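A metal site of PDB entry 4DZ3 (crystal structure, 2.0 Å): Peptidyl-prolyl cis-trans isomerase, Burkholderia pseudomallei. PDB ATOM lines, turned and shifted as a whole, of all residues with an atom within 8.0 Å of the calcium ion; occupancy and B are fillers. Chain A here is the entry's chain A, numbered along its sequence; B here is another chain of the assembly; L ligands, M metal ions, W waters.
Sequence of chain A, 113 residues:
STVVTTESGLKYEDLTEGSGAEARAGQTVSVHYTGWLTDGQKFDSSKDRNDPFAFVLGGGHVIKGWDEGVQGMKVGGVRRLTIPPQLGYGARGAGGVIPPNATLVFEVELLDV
N of Asp 51 lies within hydrogen-bond range of O of Ser 46, at 3.0 Å. The backbone carbonyl oxygen of Asp 112 of chain B lies within hydrogen-bond range of the backbone NH of Ser 30 of chain B (2.9 Å).
Of the 19 residues printed, 4 come within 4 Å of the calcium ion.
The calcium ion is bound by water W1 (2.3 Å), O of Pro 52 (2.3 Å), O of Val 113 of chain B (2.4 Å), water W2 (2.4 Å), OD1 of Asp 51 (2.4 Å), OD2 of Asp 112 of chain B (2.4 Å) and OD1 of Asp 112 of chain B (2.6 Å).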
ATOM      1  N   SER A  30       0.225 -28.309  10.643  1.00  0.00           N
ATOM      2  CA  SER A  30       0.018 -28.547  12.056  1.00  0.00           C
ATOM      3  C   SER A  30       1.045 -29.575  12.505  1.00  0.00           C
ATOM      4  O   SER A  30       1.207 -30.617  11.872  1.00  0.00           O
ATOM      5  CB  SER A  30      -1.393 -29.040  12.311  1.00  0.00           C
ATOM      6  OG  SER A  30      -1.588 -29.310  13.707  1.00  0.00           O
ATOM      7  N   VAL A  31       1.758 -29.262  13.583  1.00  0.00           N
ATOM      8  CA  VAL A  31       2.776 -30.129  14.090  1.00  0.00           C
ATOM      9  C   VAL A  31       2.718 -30.252  15.586  1.00  0.00           C
ATOM     10  O   VAL A  31       2.116 -29.396  16.285  1.00  0.00           O
ATOM     11  CB  VAL A  31       4.212 -29.598  13.730  1.00  0.00           C
ATOM     12  CG1 VAL A  31       4.341 -29.284  12.253  1.00  0.00           C
ATOM     13  CG2 VAL A  31       4.582 -28.356  14.577  1.00  0.00           C
ATOM     14  N   HIS A  32       3.337 -31.327  16.074  1.00  0.00           N
ATOM     15  CA  HIS A  32       3.786 -31.444  17.438  1.00  0.00           C
ATOM     16  C   HIS A  32       5.292 -31.325  17.371  1.00  0.00           C
ATOM     17  O   HIS A  32       5.935 -31.799  16.406  1.00  0.00           O
ATOM     18  CB  HIS A  32       3.405 -32.765  18.096  1.00  0.00           C
ATOM     19  CG  HIS A  32       2.086 -32.727  18.836  1.00  0.00           C
ATOM     20  ND1 HIS A  32       1.780 -31.765  19.720  1.00  0.00           N
ATOM     21  CD2 HIS A  32       1.012 -33.581  18.807  1.00  0.00           C
ATOM     22  CE1 HIS A  32       0.564 -31.990  20.228  1.00  0.00           C
ATOM     23  NE2 HIS A  32       0.095 -33.098  19.672  1.00  0.00           N
ATOM     24  N   SER A  46       5.122 -28.994  22.609  1.00  0.00           N
ATOM     25  CA  SER A  46       3.678 -28.814  22.356  1.00  0.00           C
ATOM     26  C   SER A  46       2.855 -29.989  22.940  1.00  0.00           C
ATOM     27  O   SER A  46       1.666 -29.800  23.293  1.00  0.00           O
ATOM     28  CB  SER A  46       3.424 -28.691  20.851  1.00  0.00           C
ATOM     29  OG  SER A  46       3.772 -29.883  20.191  1.00  0.00           O
ATOM     30  N   ARG A  49       1.764 -29.278  26.545  1.00  0.00           N
ATOM     31  CA  ARG A  49       0.607 -28.368  26.576  1.00  0.00           C
ATOM     32  C   ARG A  49      -0.660 -28.985  25.933  1.00  0.00           C
ATOM     33  O   ARG A  49      -1.740 -28.377  25.948  1.00  0.00           O
ATOM     34  CB  ARG A  49       0.960 -27.051  25.857  1.00  0.00           C
ATOM     35  CG  ARG A  49       2.036 -26.230  26.572  1.00  0.00           C
ATOM     36  CD  ARG A  49       2.326 -24.902  25.890  1.00  0.00           C
ATOM     37  NE  ARG A  49       3.410 -24.993  24.923  1.00  0.00           N
ATOM     38  CZ  ARG A  49       3.259 -25.234  23.626  1.00  0.00           C
ATOM     39  NH1 ARG A  49       4.308 -25.284  22.836  1.00  0.00           N
ATOM     40  NH2 ARG A  49       2.039 -25.413  23.122  1.00  0.00           N
ATOM     41  N   ASN A  50      -0.520 -30.198  25.357  1.00  0.00           N
ATOM     42  CA  ASN A  50      -1.599 -30.877  24.638  1.00  0.00           C
ATOM     43  C   ASN A  50      -2.178 -29.940  23.558  1.00  0.00           C
ATOM     44  O   ASN A  50      -3.382 -29.861  23.369  1.00  0.00           O
ATOM     45  CB  ASN A  50      -2.692 -31.357  25.615  1.00  0.00           C
ATOM     46  CG  ASN A  50      -3.686 -32.309  24.967  1.00  0.00           C
ATOM     47  OD1 ASN A  50      -3.434 -32.888  23.920  1.00  0.00           O
ATOM     48  ND2 ASN A  50      -4.830 -32.488  25.608  1.00  0.00           N
ATOM     49  N   ASP A  51      -1.285 -29.242  22.843  1.00  0.00           N
ATOM     50  CA  ASP A  51      -1.680 -28.190  21.946  1.00  0.00           C
ATOM     51  C   ASP A  51      -0.833 -28.186  20.668  1.00  0.00           C
ATOM     52  O   ASP A  51       0.245 -27.635  20.666  1.00  0.00           O
ATOM     53  CB  ASP A  51      -1.563 -26.837  22.677  1.00  0.00           C
ATOM     54  CG  ASP A  51      -2.126 -25.648  21.853  1.00  0.00           C
ATOM     55  OD1 ASP A  51      -2.769 -25.879  20.821  1.00  0.00           O
ATOM     56  OD2 ASP A  51      -1.922 -24.501  22.256  1.00  0.00           O
ATOM     57  N   PRO A  52      -1.344 -28.830  19.583  1.00  0.00           N
ATOM     58  CA  PRO A  52      -0.644 -28.797  18.317  1.00  0.00           C
ATOM     59  C   PRO A  52      -0.370 -27.359  17.841  1.00  0.00           C
ATOM     60  O   PRO A  52      -1.147 -26.443  18.142  1.00  0.00           O
ATOM     61  CB  PRO A  52      -1.597 -29.536  17.374  1.00  0.00           C
ATOM     62  CG  PRO A  52      -2.335 -30.479  18.254  1.00  0.00           C
ATOM     63  CD  PRO A  52      -2.520 -29.721  19.528  1.00  0.00           C
ATOM     64  N   PHE A  53       0.738 -27.198  17.108  1.00  0.00           N
ATOM     65  CA  PHE A  53       1.200 -25.884  16.686  1.00  0.00           C
ATOM     66  C   PHE A  53       0.967 -25.754  15.201  1.00  0.00           C
ATOM     67  O   PHE A  53       1.461 -26.549  14.445  1.00  0.00           O
ATOM     68  CB  PHE A  53       2.693 -25.690  17.036  1.00  0.00           C
ATOM     69  CG  PHE A  53       3.295 -24.429  16.479  1.00  0.00           C
ATOM     70  CD1 PHE A  53       2.841 -23.176  16.895  1.00  0.00           C
ATOM     71  CD2 PHE A  53       4.318 -24.488  15.522  1.00  0.00           C
ATOM     72  CE1 PHE A  53       3.386 -22.004  16.373  1.00  0.00           C
ATOM     73  CE2 PHE A  53       4.877 -23.312  15.013  1.00  0.00           C
ATOM     74  CZ  PHE A  53       4.414 -22.079  15.431  1.00  0.00           C
ATOM     75  N   ALA A  54       0.172 -24.741  14.808  1.00  0.00           N
ATOM     76  CA  ALA A  54      -0.150 -24.470  13.416  1.00  0.00           C
ATOM     77  C   ALA A  54       0.638 -23.260  12.949  1.00  0.00           C
ATOM     78  O   ALA A  54       0.775 -22.296  13.681  1.00  0.00           O
ATOM     79  CB  ALA A  54      -1.633 -24.227  13.243  1.00  0.00           C
ATOM     80  N   ALA B  21      -9.456 -25.799  24.937  1.00  0.00           N
ATOM     81  CA  ALA B  21      -9.468 -24.352  24.713  1.00  0.00           C
ATOM     82  C   ALA B  21     -10.654 -23.882  23.849  1.00  0.00           C
ATOM     83  O   ALA B  21     -11.097 -24.619  22.955  1.00  0.00           O
ATOM     84  CB  ALA B  21      -8.147 -23.896  24.079  1.00  0.00           C
ATOM     85  N   GLN B  27      -8.422 -16.833  15.643  1.00  0.00           N
ATOM     86  CA  GLN B  27      -7.662 -18.081  15.717  1.00  0.00           C
ATOM     87  C   GLN B  27      -7.753 -18.912  14.452  1.00  0.00           C
ATOM     88  O   GLN B  27      -8.779 -18.900  13.752  1.00  0.00           O
ATOM     89  CB  GLN B  27      -8.169 -18.919  16.886  1.00  0.00           C
ATOM     90  CG  GLN B  27      -7.826 -18.296  18.226  1.00  0.00           C
ATOM     91  CD  GLN B  27      -8.338 -19.121  19.397  1.00  0.00           C
ATOM     92  OE1 GLN B  27      -9.376 -19.711  19.323  1.00  0.00           O
ATOM     93  NE2 GLN B  27      -7.587 -19.131  20.478  1.00  0.00           N
ATOM     94  N   THR B  28      -6.672 -19.648  14.163  1.00  0.00           N
ATOM     95  CA  THR B  28      -6.682 -20.603  13.071  1.00  0.00           C
ATOM     96  C   THR B  28      -7.105 -21.918  13.712  1.00  0.00           C
ATOM     97  O   THR B  28      -6.404 -22.422  14.556  1.00  0.00           O
ATOM     98  CB  THR B  28      -5.308 -20.736  12.399  1.00  0.00           C
ATOM     99  OG1 THR B  28      -4.947 -19.477  11.817  1.00  0.00           O
ATOM    100  CG2 THR B  28      -5.317 -21.857  11.307  1.00  0.00           C
ATOM    101  N   VAL B  29      -8.255 -22.444  13.306  1.00  0.00           N
ATOM    102  CA  VAL B  29      -8.795 -23.638  13.923  1.00  0.00           C
ATOM    103  C   VAL B  29      -8.705 -24.819  12.959  1.00  0.00           C
ATOM    104  O   VAL B  29      -8.624 -24.619  11.747  1.00  0.00           O
ATOM    105  CB  VAL B  29     -10.261 -23.434  14.378  1.00  0.00           C
ATOM    106  CG1 VAL B  29     -10.354 -22.198  15.293  1.00  0.00           C
ATOM    107  CG2 VAL B  29     -11.221 -23.308  13.177  1.00  0.00           C
ATOM    108  N   SER B  30      -8.714 -26.029  13.518  1.00  0.00           N
ATOM    109  CA  SER B  30      -8.702 -27.280  12.744  1.00  0.00           C
ATOM    110  C   SER B  30      -9.914 -28.106  13.151  1.00  0.00           C
ATOM    111  O   SER B  30     -10.178 -28.288  14.343  1.00  0.00           O
ATOM    112  CB  SER B  30      -7.388 -28.033  12.956  1.00  0.00           C
ATOM    113  OG  SER B  30      -7.453 -29.333  12.395  1.00  0.00           O
ATOM    114  N   VAL B  75     -12.216 -27.249  22.322  1.00  0.00           N
ATOM    115  CA  VAL B  75     -11.520 -28.348  21.641  1.00  0.00           C
ATOM    116  C   VAL B  75     -12.049 -29.672  22.218  1.00  0.00           C
ATOM    117  O   VAL B  75     -12.197 -29.818  23.438  1.00  0.00           O
ATOM    118  CB  VAL B  75      -9.970 -28.197  21.745  1.00  0.00           C
ATOM    119  CG1 VAL B  75      -9.256 -29.415  21.166  1.00  0.00           C
ATOM    120  CG2 VAL B  75      -9.513 -26.921  21.005  1.00  0.00           C
ATOM    121  N   LEU B 111     -10.793 -29.807  16.520  1.00  0.00           N
ATOM    122  CA  LEU B 111      -9.552 -30.584  16.808  1.00  0.00           C
ATOM    123  C   LEU B 111      -8.505 -29.773  17.497  1.00  0.00           C
ATOM    124  O   LEU B 111      -7.796 -30.284  18.306  1.00  0.00           O
ATOM    125  CB  LEU B 111      -8.978 -31.167  15.529  1.00  0.00           C
ATOM    126  CG  LEU B 111      -9.990 -32.006  14.719  1.00  0.00           C
ATOM    127  CD1 LEU B 111      -9.392 -32.384  13.383  1.00  0.00           C
ATOM    128  CD2 LEU B 111     -10.439 -33.267  15.492  1.00  0.00           C
ATOM    129  N   ASP B 112      -8.428 -28.471  17.168  1.00  0.00           N
ATOM    130  CA  ASP B 112      -7.402 -27.597  17.703  1.00  0.00           C
ATOM    131  C   ASP B 112      -7.737 -26.128  17.398  1.00  0.00           C
ATOM    132  O   ASP B 112      -8.482 -25.834  16.451  1.00  0.00           O
ATOM    133  CB  ASP B 112      -6.038 -27.953  17.049  1.00  0.00           C
ATOM    134  CG  ASP B 112      -4.872 -27.180  17.652  1.00  0.00           C
ATOM    135  OD1 ASP B 112      -4.782 -27.100  18.877  1.00  0.00           O
ATOM    136  OD2 ASP B 112      -4.017 -26.628  16.882  1.00  0.00           O
ATOM    137  N   VAL B 113      -7.203 -25.231  18.223  1.00  0.00           N
ATOM    138  CA  VAL B 113      -7.293 -23.781  18.039  1.00  0.00           C
ATOM    139  C   VAL B 113      -5.920 -23.147  18.265  1.00  0.00           C
ATOM    140  O   VAL B 113      -4.957 -23.825  18.669  1.00  0.00           O
ATOM    141  CB  VAL B 113      -8.289 -23.107  19.012  1.00  0.00           C
ATOM    142  CG1 VAL B 113      -9.651 -23.757  18.918  1.00  0.00           C
ATOM    143  CG2 VAL B 113      -7.751 -23.147  20.463  1.00  0.00           C
ATOM    144  OXT VAL B 113      -5.745 -21.930  18.058  1.00  0.00           O
HETATM  145  C1  LIG L   1       9.525 -20.243  16.835  1.00  0.00           C
HETATM  146  C2  LIG L   1       9.937 -21.628  17.239  1.00  0.00           C
HETATM  147  C3  LIG L   1       9.526 -22.624  16.176  1.00  0.00           C
HETATM  148  C4  LIG L   1       8.060 -22.955  16.154  1.00  0.00           C
HETATM  149  C5  LIG L   1       7.682 -23.491  17.515  1.00  0.00           C
HETATM  150  C6  LIG L   1       7.929 -22.419  18.546  1.00  0.00           C
HETATM  151  C7  LIG L   1      10.271 -22.229  19.605  1.00  0.00           C
HETATM  152  C8  LIG L   1       9.806 -22.689  20.924  1.00  0.00           C
HETATM  153  C9  LIG L   1       9.307 -21.724  21.991  1.00  0.00           C
HETATM  154  C10 LIG L   1       9.981 -20.347  22.050  1.00  0.00           C
HETATM  155  C11 LIG L   1       9.154 -19.350  22.914  1.00  0.00           C
HETATM  156  C12 LIG L   1       7.688 -19.304  22.443  1.00  0.00           C
HETATM  157  C13 LIG L   1       7.142 -20.747  22.482  1.00  0.00           C
HETATM  158  C14 LIG L   1       5.675 -20.991  22.030  1.00  0.00           C
HETATM  159  C15 LIG L   1       5.356 -20.400  20.636  1.00  0.00           C
HETATM  160  C16 LIG L   1       3.977 -20.823  20.031  1.00  0.00           C
HETATM  161  C17 LIG L   1       2.777 -20.011  20.577  1.00  0.00           C
HETATM  162  C18 LIG L   1       2.749 -18.668  19.918  1.00  0.00           C
HETATM  163  C19 LIG L   1       3.361 -17.631  20.512  1.00  0.00           C
HETATM  164  C20 LIG L   1       3.399 -16.235  19.928  1.00  0.00           C
HETATM  165  C21 LIG L   1       4.761 -16.071  19.296  1.00  0.00           C
HETATM  166  C22 LIG L   1       4.853 -16.240  17.796  1.00  0.00           C
HETATM  167  C23 LIG L   1       6.277 -16.528  17.297  1.00  0.00           C
HETATM  168  C24 LIG L   1       6.822 -17.936  17.653  1.00  0.00           C
HETATM  169  C25 LIG L   1       8.300 -18.153  17.267  1.00  0.00           C
HETATM  170  C26 LIG L   1       9.193 -17.144  17.899  1.00  0.00           C
HETATM  171  C27 LIG L   1       9.893 -16.313  17.057  1.00  0.00           C
HETATM  172  C28 LIG L   1      10.822 -15.229  17.527  1.00  0.00           C
HETATM  173  C29 LIG L   1      12.053 -15.147  16.625  1.00  0.00           C
HETATM  174  C30 LIG L   1      12.927 -13.903  16.881  1.00  0.00           C
HETATM  175  C31 LIG L   1      12.127 -12.604  16.956  1.00  0.00           C
HETATM  176  C32 LIG L   1      10.845 -12.706  17.783  1.00  0.00           C
HETATM  177  C33 LIG L   1      10.015 -13.941  17.506  1.00  0.00           C
HETATM  178  C34 LIG L   1      11.424 -20.497  22.508  1.00  0.00           C
HETATM  179  C35 LIG L   1       3.694 -22.323  20.232  1.00  0.00           C
HETATM  180  C36 LIG L   1       2.022 -18.568  18.608  1.00  0.00           C
HETATM  181  C37 LIG L   1       3.123 -15.222  21.022  1.00  0.00           C
HETATM  182  C38 LIG L   1       3.596 -13.872  20.559  1.00  0.00           C
HETATM  183  C39 LIG L   1       2.888 -13.083  19.801  1.00  0.00           C
HETATM  184  C40 LIG L   1       6.002 -19.013  16.982  1.00  0.00           C
HETATM  185  C41 LIG L   1       9.255 -17.093  19.412  1.00  0.00           C
HETATM  186  C42 LIG L   1       7.091 -17.039  23.006  1.00  0.00           C
HETATM  187  C43 LIG L   1       4.610 -21.382  24.143  1.00  0.00           C
HETATM  188  C44 LIG L   1      14.948 -14.735  15.802  1.00  0.00           C
HETATM  189  N1  LIG L   1       9.392 -22.121  18.568  1.00  0.00           N
HETATM  190  O1  LIG L   1       8.689 -19.451  17.710  1.00  0.00           O
HETATM  191  O2  LIG L   1       9.920 -19.817  15.760  1.00  0.00           O
HETATM  192  O3  LIG L   1      11.468 -21.986  19.510  1.00  0.00           O
HETATM  193  O4  LIG L   1       9.858 -23.894  21.151  1.00  0.00           O
HETATM  194  O5  LIG L   1       7.942 -21.554  21.639  1.00  0.00           O
HETATM  195  O6  LIG L   1       9.454 -22.350  23.280  1.00  0.00           O
HETATM  196  O7  LIG L   1       6.866 -18.435  23.227  1.00  0.00           O
HETATM  197  O8  LIG L   1       4.794 -20.480  23.030  1.00  0.00           O
HETATM  198  O9  LIG L   1       5.752 -15.808  19.962  1.00  0.00           O
HETATM  199  O10 LIG L   1       6.265 -16.372  15.881  1.00  0.00           O
HETATM  200  O11 LIG L   1      13.889 -13.758  15.807  1.00  0.00           O
HETATM  201  O12 LIG L   1      12.933 -11.622  17.587  1.00  0.00           O
HETATM  202 CA    CA M   1      -3.018 -25.177  18.569  1.00  0.00          CA
HETATM  203  O   HOH W   1      -2.402 -24.055  16.679  1.00  0.00           O
HETATM  204  O   HOH W   2      -2.068 -23.279  19.619  1.00  0.00           O
